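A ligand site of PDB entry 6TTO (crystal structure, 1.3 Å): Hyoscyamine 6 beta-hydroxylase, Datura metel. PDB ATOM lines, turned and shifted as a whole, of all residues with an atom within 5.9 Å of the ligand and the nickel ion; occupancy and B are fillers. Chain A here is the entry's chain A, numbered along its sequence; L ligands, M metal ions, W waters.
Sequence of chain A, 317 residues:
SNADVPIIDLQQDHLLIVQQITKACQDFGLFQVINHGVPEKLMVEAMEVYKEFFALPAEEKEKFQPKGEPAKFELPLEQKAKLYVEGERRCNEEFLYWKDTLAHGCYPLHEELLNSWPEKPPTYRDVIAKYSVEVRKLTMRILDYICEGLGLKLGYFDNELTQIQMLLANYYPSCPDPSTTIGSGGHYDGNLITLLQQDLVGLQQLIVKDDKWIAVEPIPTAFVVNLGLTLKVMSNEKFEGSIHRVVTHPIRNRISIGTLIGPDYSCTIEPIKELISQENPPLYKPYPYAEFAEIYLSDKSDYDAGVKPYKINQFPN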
ATOM      1  N   LYS A  99     -16.455  -3.122 -11.378  1.00  0.00           N
ATOM      2  CA  LYS A  99     -17.114  -4.389 -11.107  1.00  0.00           C
ATOM      3  C   LYS A  99     -17.678  -4.320  -9.697  1.00  0.00           C
ATOM      4  O   LYS A  99     -16.936  -4.054  -8.752  1.00  0.00           O
ATOM      5  CB  LYS A  99     -16.096  -5.521 -11.192  1.00  0.00           C
ATOM      6  CG  LYS A  99     -16.604  -6.887 -10.770  1.00  0.00           C
ATOM      7  CD  LYS A  99     -15.440  -7.830 -10.531  1.00  0.00           C
ATOM      8  CE  LYS A  99     -15.940  -9.130  -9.922  1.00  0.00           C
ATOM      9  NZ  LYS A  99     -14.937  -9.837  -9.094  1.00  0.00           N
ATOM     10  N   LEU A 168     -21.266 -14.659  -3.780  1.00  0.00           N
ATOM     11  CA  LEU A 168     -20.769 -13.456  -4.471  1.00  0.00           C
ATOM     12  C   LEU A 168     -21.627 -13.246  -5.704  1.00  0.00           C
ATOM     13  O   LEU A 168     -21.556 -14.055  -6.642  1.00  0.00           O
ATOM     14  CB  LEU A 168     -19.330 -13.603  -4.876  1.00  0.00           C
ATOM     15  CG  LEU A 168     -18.267 -13.242  -3.817  1.00  0.00           C
ATOM     16  CD1 LEU A 168     -18.331 -14.105  -2.589  1.00  0.00           C
ATOM     17  CD2 LEU A 168     -16.895 -13.271  -4.458  1.00  0.00           C
ATOM     18  N   ASN A 170     -22.008 -10.984  -8.730  1.00  0.00           N
ATOM     19  CA  ASN A 170     -21.203 -10.013  -9.467  1.00  0.00           C
ATOM     20  C   ASN A 170     -22.042  -9.308 -10.494  1.00  0.00           C
ATOM     21  O   ASN A 170     -22.962  -9.881 -11.109  1.00  0.00           O
ATOM     22  CB  ASN A 170     -20.058 -10.747 -10.146  1.00  0.00           C
ATOM     23  CG  ASN A 170     -19.313 -11.609  -9.185  1.00  0.00           C
ATOM     24  OD1 ASN A 170     -18.725 -11.125  -8.220  1.00  0.00           O
ATOM     25  ND2 ASN A 170     -19.387 -12.908  -9.403  1.00  0.00           N
ATOM     26  N   TYR A 172     -21.311  -6.804 -13.823  1.00  0.00           N
ATOM     27  CA  TYR A 172     -20.322  -6.304 -14.759  1.00  0.00           C
ATOM     28  C   TYR A 172     -21.015  -5.335 -15.702  1.00  0.00           C
ATOM     29  O   TYR A 172     -21.727  -5.766 -16.624  1.00  0.00           O
ATOM     30  CB  TYR A 172     -19.693  -7.464 -15.555  1.00  0.00           C
ATOM     31  CG  TYR A 172     -19.071  -8.552 -14.703  1.00  0.00           C
ATOM     32  CD1 TYR A 172     -19.827  -9.651 -14.284  1.00  0.00           C
ATOM     33  CD2 TYR A 172     -17.739  -8.524 -14.374  1.00  0.00           C
ATOM     34  CE1 TYR A 172     -19.251 -10.656 -13.523  1.00  0.00           C
ATOM     35  CE2 TYR A 172     -17.172  -9.525 -13.611  1.00  0.00           C
ATOM     36  CZ  TYR A 172     -17.908 -10.595 -13.219  1.00  0.00           C
ATOM     37  OH  TYR A 172     -17.278 -11.563 -12.435  1.00  0.00           O
ATOM     38  N   SER A 184     -13.017  -8.830 -14.890  1.00  0.00           N
ATOM     39  CA  SER A 184     -12.420  -9.548 -13.762  1.00  0.00           C
ATOM     40  C   SER A 184     -11.183 -10.301 -14.258  1.00  0.00           C
ATOM     41  O   SER A 184     -11.289 -11.239 -15.054  1.00  0.00           O
ATOM     42  CB  SER A 184     -13.439 -10.516 -13.159  1.00  0.00           C
ATOM     43  OG  SER A 184     -12.944 -11.094 -11.961  1.00  0.00           O
ATOM     44  N   HIS A 187      -7.675 -15.467 -12.478  1.00  0.00           N
ATOM     45  CA  HIS A 187      -7.366 -15.882 -11.116  1.00  0.00           C
ATOM     46  C   HIS A 187      -7.744 -17.346 -10.953  1.00  0.00           C
ATOM     47  O   HIS A 187      -8.590 -17.880 -11.679  1.00  0.00           O
ATOM     48  CB  HIS A 187      -8.145 -15.086 -10.067  1.00  0.00           C
ATOM     49  CG  HIS A 187      -9.633 -15.218 -10.198  1.00  0.00           C
ATOM     50  ND1 HIS A 187     -10.359 -14.554 -11.172  1.00  0.00           N
ATOM     51  CD2 HIS A 187     -10.532 -15.976  -9.520  1.00  0.00           C
ATOM     52  CE1 HIS A 187     -11.633 -14.897 -11.071  1.00  0.00           C
ATOM     53  NE2 HIS A 187     -11.773 -15.721 -10.053  1.00  0.00           N
ATOM     54  N   TYR A 188      -7.109 -17.989  -9.976  1.00  0.00           N
ATOM     55  CA  TYR A 188      -7.713 -19.124  -9.313  1.00  0.00           C
ATOM     56  C   TYR A 188      -8.620 -18.576  -8.222  1.00  0.00           C
ATOM     57  O   TYR A 188      -8.296 -17.540  -7.630  1.00  0.00           O
ATOM     58  CB  TYR A 188      -6.702 -19.959  -8.544  1.00  0.00           C
ATOM     59  CG  TYR A 188      -5.673 -20.747  -9.296  1.00  0.00           C
ATOM     60  CD1 TYR A 188      -5.964 -22.017  -9.797  1.00  0.00           C
ATOM     61  CD2 TYR A 188      -4.350 -20.293  -9.399  1.00  0.00           C
ATOM     62  CE1 TYR A 188      -4.984 -22.771 -10.414  1.00  0.00           C
ATOM     63  CE2 TYR A 188      -3.375 -21.032 -10.022  1.00  0.00           C
ATOM     64  CZ  TYR A 188      -3.684 -22.273 -10.506  1.00  0.00           C
ATOM     65  OH  TYR A 188      -2.715 -23.036 -11.103  1.00  0.00           O
ATOM     66  N   ASP A 189      -9.703 -19.271  -7.915  1.00  0.00           N
ATOM     67  CA  ASP A 189     -10.403 -19.042  -6.664  1.00  0.00           C
ATOM     68  C   ASP A 189      -9.542 -19.618  -5.540  1.00  0.00           C
ATOM     69  O   ASP A 189      -8.847 -20.609  -5.730  1.00  0.00           O
ATOM     70  CB  ASP A 189     -11.781 -19.722  -6.666  1.00  0.00           C
ATOM     71  CG  ASP A 189     -12.774 -19.047  -7.604  1.00  0.00           C
ATOM     72  OD1 ASP A 189     -12.433 -18.036  -8.240  1.00  0.00           O
ATOM     73  OD2 ASP A 189     -13.931 -19.530  -7.676  1.00  0.00           O
ATOM     74  N   THR A 194     -16.083 -23.879  -6.040  1.00  0.00           N
ATOM     75  CA  THR A 194     -17.027 -22.817  -6.345  1.00  0.00           C
ATOM     76  C   THR A 194     -18.041 -23.333  -7.360  1.00  0.00           C
ATOM     77  O   THR A 194     -17.667 -23.982  -8.322  1.00  0.00           O
ATOM     78  CB  THR A 194     -16.271 -21.622  -6.938  1.00  0.00           C
ATOM     79  OG1 THR A 194     -15.393 -21.128  -5.936  1.00  0.00           O
ATOM     80  CG2 THR A 194     -17.230 -20.524  -7.348  1.00  0.00           C
ATOM     81  N   LEU A 196     -20.927 -21.676  -9.922  1.00  0.00           N
ATOM     82  CA  LEU A 196     -21.205 -20.390 -10.547  1.00  0.00           C
ATOM     83  C   LEU A 196     -22.382 -20.533 -11.499  1.00  0.00           C
ATOM     84  O   LEU A 196     -22.390 -21.414 -12.384  1.00  0.00           O
ATOM     85  CB  LEU A 196     -19.942 -19.934 -11.281  1.00  0.00           C
ATOM     86  CG  LEU A 196     -19.793 -18.580 -11.929  1.00  0.00           C
ATOM     87  CD1 LEU A 196     -20.586 -18.486 -13.194  1.00  0.00           C
ATOM     88  CD2 LEU A 196     -20.076 -17.455 -10.987  1.00  0.00           C
ATOM     89  N   GLN A 198     -24.494 -18.597 -14.409  1.00  0.00           N
ATOM     90  CA  GLN A 198     -24.376 -17.523 -15.381  1.00  0.00           C
ATOM     91  C   GLN A 198     -25.403 -17.734 -16.494  1.00  0.00           C
ATOM     92  O   GLN A 198     -25.849 -18.859 -16.745  1.00  0.00           O
ATOM     93  CB  GLN A 198     -22.970 -17.459 -16.006  1.00  0.00           C
ATOM     94  CG  GLN A 198     -22.560 -18.777 -16.631  1.00  0.00           C
ATOM     95  CD  GLN A 198     -21.379 -18.684 -17.578  1.00  0.00           C
ATOM     96  OE1 GLN A 198     -20.791 -17.594 -17.799  1.00  0.00           O
ATOM     97  NE2 GLN A 198     -20.983 -19.818 -18.132  1.00  0.00           N
ATOM     98  N   LEU A 203     -17.398 -15.552 -19.338  1.00  0.00           N
ATOM     99  CA  LEU A 203     -16.489 -16.375 -18.548  1.00  0.00           C
ATOM    100  C   LEU A 203     -15.556 -17.155 -19.474  1.00  0.00           C
ATOM    101  O   LEU A 203     -16.009 -17.783 -20.440  1.00  0.00           O
ATOM    102  CB  LEU A 203     -17.258 -17.315 -17.633  1.00  0.00           C
ATOM    103  CG  LEU A 203     -16.426 -18.192 -16.703  1.00  0.00           C
ATOM    104  CD1 LEU A 203     -15.650 -17.393 -15.678  1.00  0.00           C
ATOM    105  CD2 LEU A 203     -17.379 -19.172 -16.016  1.00  0.00           C
ATOM    106  N   ASN A 226     -15.847 -24.964 -10.396  1.00  0.00           N
ATOM    107  CA  ASN A 226     -14.420 -24.777 -10.545  1.00  0.00           C
ATOM    108  C   ASN A 226     -13.708 -24.998  -9.229  1.00  0.00           C
ATOM    109  O   ASN A 226     -14.146 -24.561  -8.163  1.00  0.00           O
ATOM    110  CB  ASN A 226     -14.066 -23.449 -11.166  1.00  0.00           C
ATOM    111  CG  ASN A 226     -14.395 -22.302 -10.288  1.00  0.00           C
ATOM    112  OD1 ASN A 226     -15.528 -21.832 -10.281  1.00  0.00           O
ATOM    113  ND2 ASN A 226     -13.420 -21.835  -9.536  1.00  0.00           N
ATOM    114  N   HIS A 244      -9.461 -18.698 -14.372  1.00  0.00           N
ATOM    115  CA  HIS A 244     -10.571 -18.192 -15.171  1.00  0.00           C
ATOM    116  C   HIS A 244     -10.600 -16.677 -15.072  1.00  0.00           C
ATOM    117  O   HIS A 244      -9.985 -16.081 -14.179  1.00  0.00           O
ATOM    118  CB  HIS A 244     -11.907 -18.851 -14.752  1.00  0.00           C
ATOM    119  CG  HIS A 244     -12.167 -18.750 -13.280  1.00  0.00           C
ATOM    120  ND1 HIS A 244     -11.672 -19.629 -12.362  1.00  0.00           N
ATOM    121  CD2 HIS A 244     -12.875 -17.829 -12.570  1.00  0.00           C
ATOM    122  CE1 HIS A 244     -12.052 -19.268 -11.153  1.00  0.00           C
ATOM    123  NE2 HIS A 244     -12.756 -18.157 -11.244  1.00  0.00           N
ATOM    124  N   ARG A 245     -11.316 -16.058 -16.005  1.00  0.00           N
ATOM    125  CA  ARG A 245     -11.444 -14.606 -16.044  1.00  0.00           C
ATOM    126  C   ARG A 245     -12.793 -14.263 -16.652  1.00  0.00           C
ATOM    127  O   ARG A 245     -13.457 -15.109 -17.255  1.00  0.00           O
ATOM    128  CB  ARG A 245     -10.321 -13.953 -16.877  1.00  0.00           C
ATOM    129  CG  ARG A 245     -10.471 -14.151 -18.394  1.00  0.00           C
ATOM    130  CD  ARG A 245      -9.281 -13.620 -19.167  1.00  0.00           C
ATOM    131  NE  ARG A 245      -9.469 -13.791 -20.603  1.00  0.00           N
ATOM    132  CZ  ARG A 245      -8.577 -13.438 -21.521  1.00  0.00           C
ATOM    133  NH1 ARG A 245      -7.434 -12.886 -21.156  1.00  0.00           N
ATOM    134  NH2 ARG A 245      -8.834 -13.645 -22.814  1.00  0.00           N
ATOM    135  N   VAL A 246     -13.167 -12.998 -16.544  1.00  0.00           N
ATOM    136  CA  VAL A 246     -14.418 -12.492 -17.136  1.00  0.00           C
ATOM    137  C   VAL A 246     -14.129 -11.326 -18.073  1.00  0.00           C
ATOM    138  O   VAL A 246     -13.437 -10.378 -17.686  1.00  0.00           O
ATOM    139  CB  VAL A 246     -15.441 -12.083 -16.085  1.00  0.00           C
ATOM    140  CG1 VAL A 246     -16.712 -11.501 -16.741  1.00  0.00           C
ATOM    141  CG2 VAL A 246     -15.806 -13.268 -15.217  1.00  0.00           C
ATOM    142  N   ARG A 254     -23.812  -7.922 -17.236  1.00  0.00           N
ATOM    143  CA  ARG A 254     -23.815  -9.337 -16.911  1.00  0.00           C
ATOM    144  C   ARG A 254     -23.843  -9.522 -15.408  1.00  0.00           C
ATOM    145  O   ARG A 254     -23.123  -8.848 -14.682  1.00  0.00           O
ATOM    146  CB  ARG A 254     -22.550  -9.982 -17.458  1.00  0.00           C
ATOM    147  CG  ARG A 254     -22.437 -11.489 -17.184  1.00  0.00           C
ATOM    148  CD  ARG A 254     -21.254 -12.082 -17.939  1.00  0.00           C
ATOM    149  NE  ARG A 254     -21.014 -13.502 -17.616  1.00  0.00           N
ATOM    150  CZ  ARG A 254     -20.369 -13.921 -16.531  1.00  0.00           C
ATOM    151  NH1 ARG A 254     -19.874 -13.035 -15.678  1.00  0.00           N
ATOM    152  NH2 ARG A 254     -20.235 -15.218 -16.295  1.00  0.00           N
ATOM    153  N   SER A 256     -23.482 -12.665 -12.497  1.00  0.00           N
ATOM    154  CA  SER A 256     -23.247 -14.074 -12.161  1.00  0.00           C
ATOM    155  C   SER A 256     -23.414 -14.268 -10.669  1.00  0.00           C
ATOM    156  O   SER A 256     -23.258 -13.344  -9.870  1.00  0.00           O
ATOM    157  CB  SER A 256     -21.867 -14.514 -12.593  1.00  0.00           C
ATOM    158  OG  SER A 256     -20.899 -13.779 -11.876  1.00  0.00           O
ATOM    159  N   LEU A 260     -19.031 -19.815  -3.126  1.00  0.00           N
ATOM    160  CA  LEU A 260     -17.641 -20.115  -2.883  1.00  0.00           C
ATOM    161  C   LEU A 260     -17.529 -20.795  -1.518  1.00  0.00           C
ATOM    162  O   LEU A 260     -17.694 -20.139  -0.471  1.00  0.00           O
ATOM    163  CB  LEU A 260     -16.803 -18.834  -2.890  1.00  0.00           C
ATOM    164  CG  LEU A 260     -16.496 -18.210  -4.262  1.00  0.00           C
ATOM    165  CD1 LEU A 260     -17.714 -17.674  -4.932  1.00  0.00           C
ATOM    166  CD2 LEU A 260     -15.415 -17.120  -4.106  1.00  0.00           C
HETATM  167  C1  LIG L   1     -15.287 -15.118  -8.915  1.00  0.00           C
HETATM  168  O1  LIG L   1     -14.328 -15.692  -8.342  1.00  0.00           O
HETATM  169  O2  LIG L   1     -16.074 -14.358  -8.293  1.00  0.00           O
HETATM  170  C2  LIG L   1     -15.516 -15.387 -10.388  1.00  0.00           C
HETATM  171  O3  LIG L   1     -14.654 -15.959 -11.007  1.00  0.00           O
HETATM  172  C3  LIG L   1     -16.821 -14.921 -11.056  1.00  0.00           C
HETATM  173  C4  LIG L   1     -16.858 -15.425 -12.483  1.00  0.00           C
HETATM  174  C5  LIG L   1     -18.074 -14.937 -13.267  1.00  0.00           C
HETATM  175  O4  LIG L   1     -18.574 -15.703 -14.083  1.00  0.00           O
HETATM  176  O5  LIG L   1     -18.565 -13.804 -13.105  1.00  0.00           O
HETATM  177 NI    NI M   1     -13.400 -16.949  -9.688  1.00  0.00          NI
HETATM  178  O   HOH W   1     -12.910 -15.376  -5.979  1.00  0.00           O
HETATM  179  O   HOH W   2     -16.307 -11.759  -7.626  1.00  0.00           O
HETATM  180  O   HOH W   3     -15.115 -18.208  -9.424  1.00  0.00           O
HETATM  181  O   HOH W   4     -14.055 -12.793  -6.590  1.00  0.00           O
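OG of Ser 256 is in hydrogen-bond range of O5 of the ligand, 2.6 Å away.
An oxygen (O4) of the ligand is in salt-bridge range of the guanidinium group (NH2) of Arg 254 (2.8 Å).
OH of Tyr 172 lies within hydrogen-bond range of O5 of the ligand (2.7 Å).
The backbone NH (N) of Tyr 172 sits at hydrogen-bond distance from the backbone carbonyl oxygen (O) of Arg 254, 2.9 Å away.
The side-chain carboxylate of Asp 189 is in hydrogen-bond range of the side-chain amide nitrogen of Asn 226, 3.0 Å away.
NH2 of Arg 254 lies within hydrogen-bond range of OE1 of Gln 198, 2.9 Å away.
OG1 of Thr 194 lies within hydrogen-bond range of OD2 of Asp 189, at 2.8 Å.
The backbone NH (N) of Val 246 is in hydrogen-bond range of the backbone carbonyl oxygen (O) of Ser 184.
The backbone NH (N) of Asn 170 lies within hydrogen-bond range of the backbone carbonyl oxygen (O) of Ser 256 (2.9 Å).
Asn 170 touches the ligand.
CD1 of Leu 196 touches O4 of the ligand (3.5 Å).
Leu 203 touches the ligand (CD1 to O4, 3.7 Å).
Val 246 touches the ligand (CG2 to C5, 3.4 Å).
Ten residues have an atom within 4 Å of the ligand: Asn 170, Tyr 172, His 187, Asp 189, Leu 196, Leu 203, His 244, Val 246, Arg 254 and Ser 256.
Along chain A the residues within 4 Å of the ligand span positions 170 to 256.
Within 4 Å of the nickel ion: His 187, Asp 189 and His 244.
The nickel ion is bound by the side-chain carboxylate of Asp 189 (2.1 Å), an oxygen (O1) of the ligand (2.1 Å), a ring nitrogen (NE2) of His 187 (2.1 Å), a ring nitrogen (NE2) of His 244 (2.1 Å), an oxygen (O3) of the ligand (2.1 Å) and water W3 (2.1 Å).
The nickel ion has six donor atoms within binding distance.
Water W2 lies within hydrogen-bond range of OD1 of Asn 170 (2.6 Å), O2 of the ligand (2.7 Å) and NZ of Lys 99 (2.8 Å).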
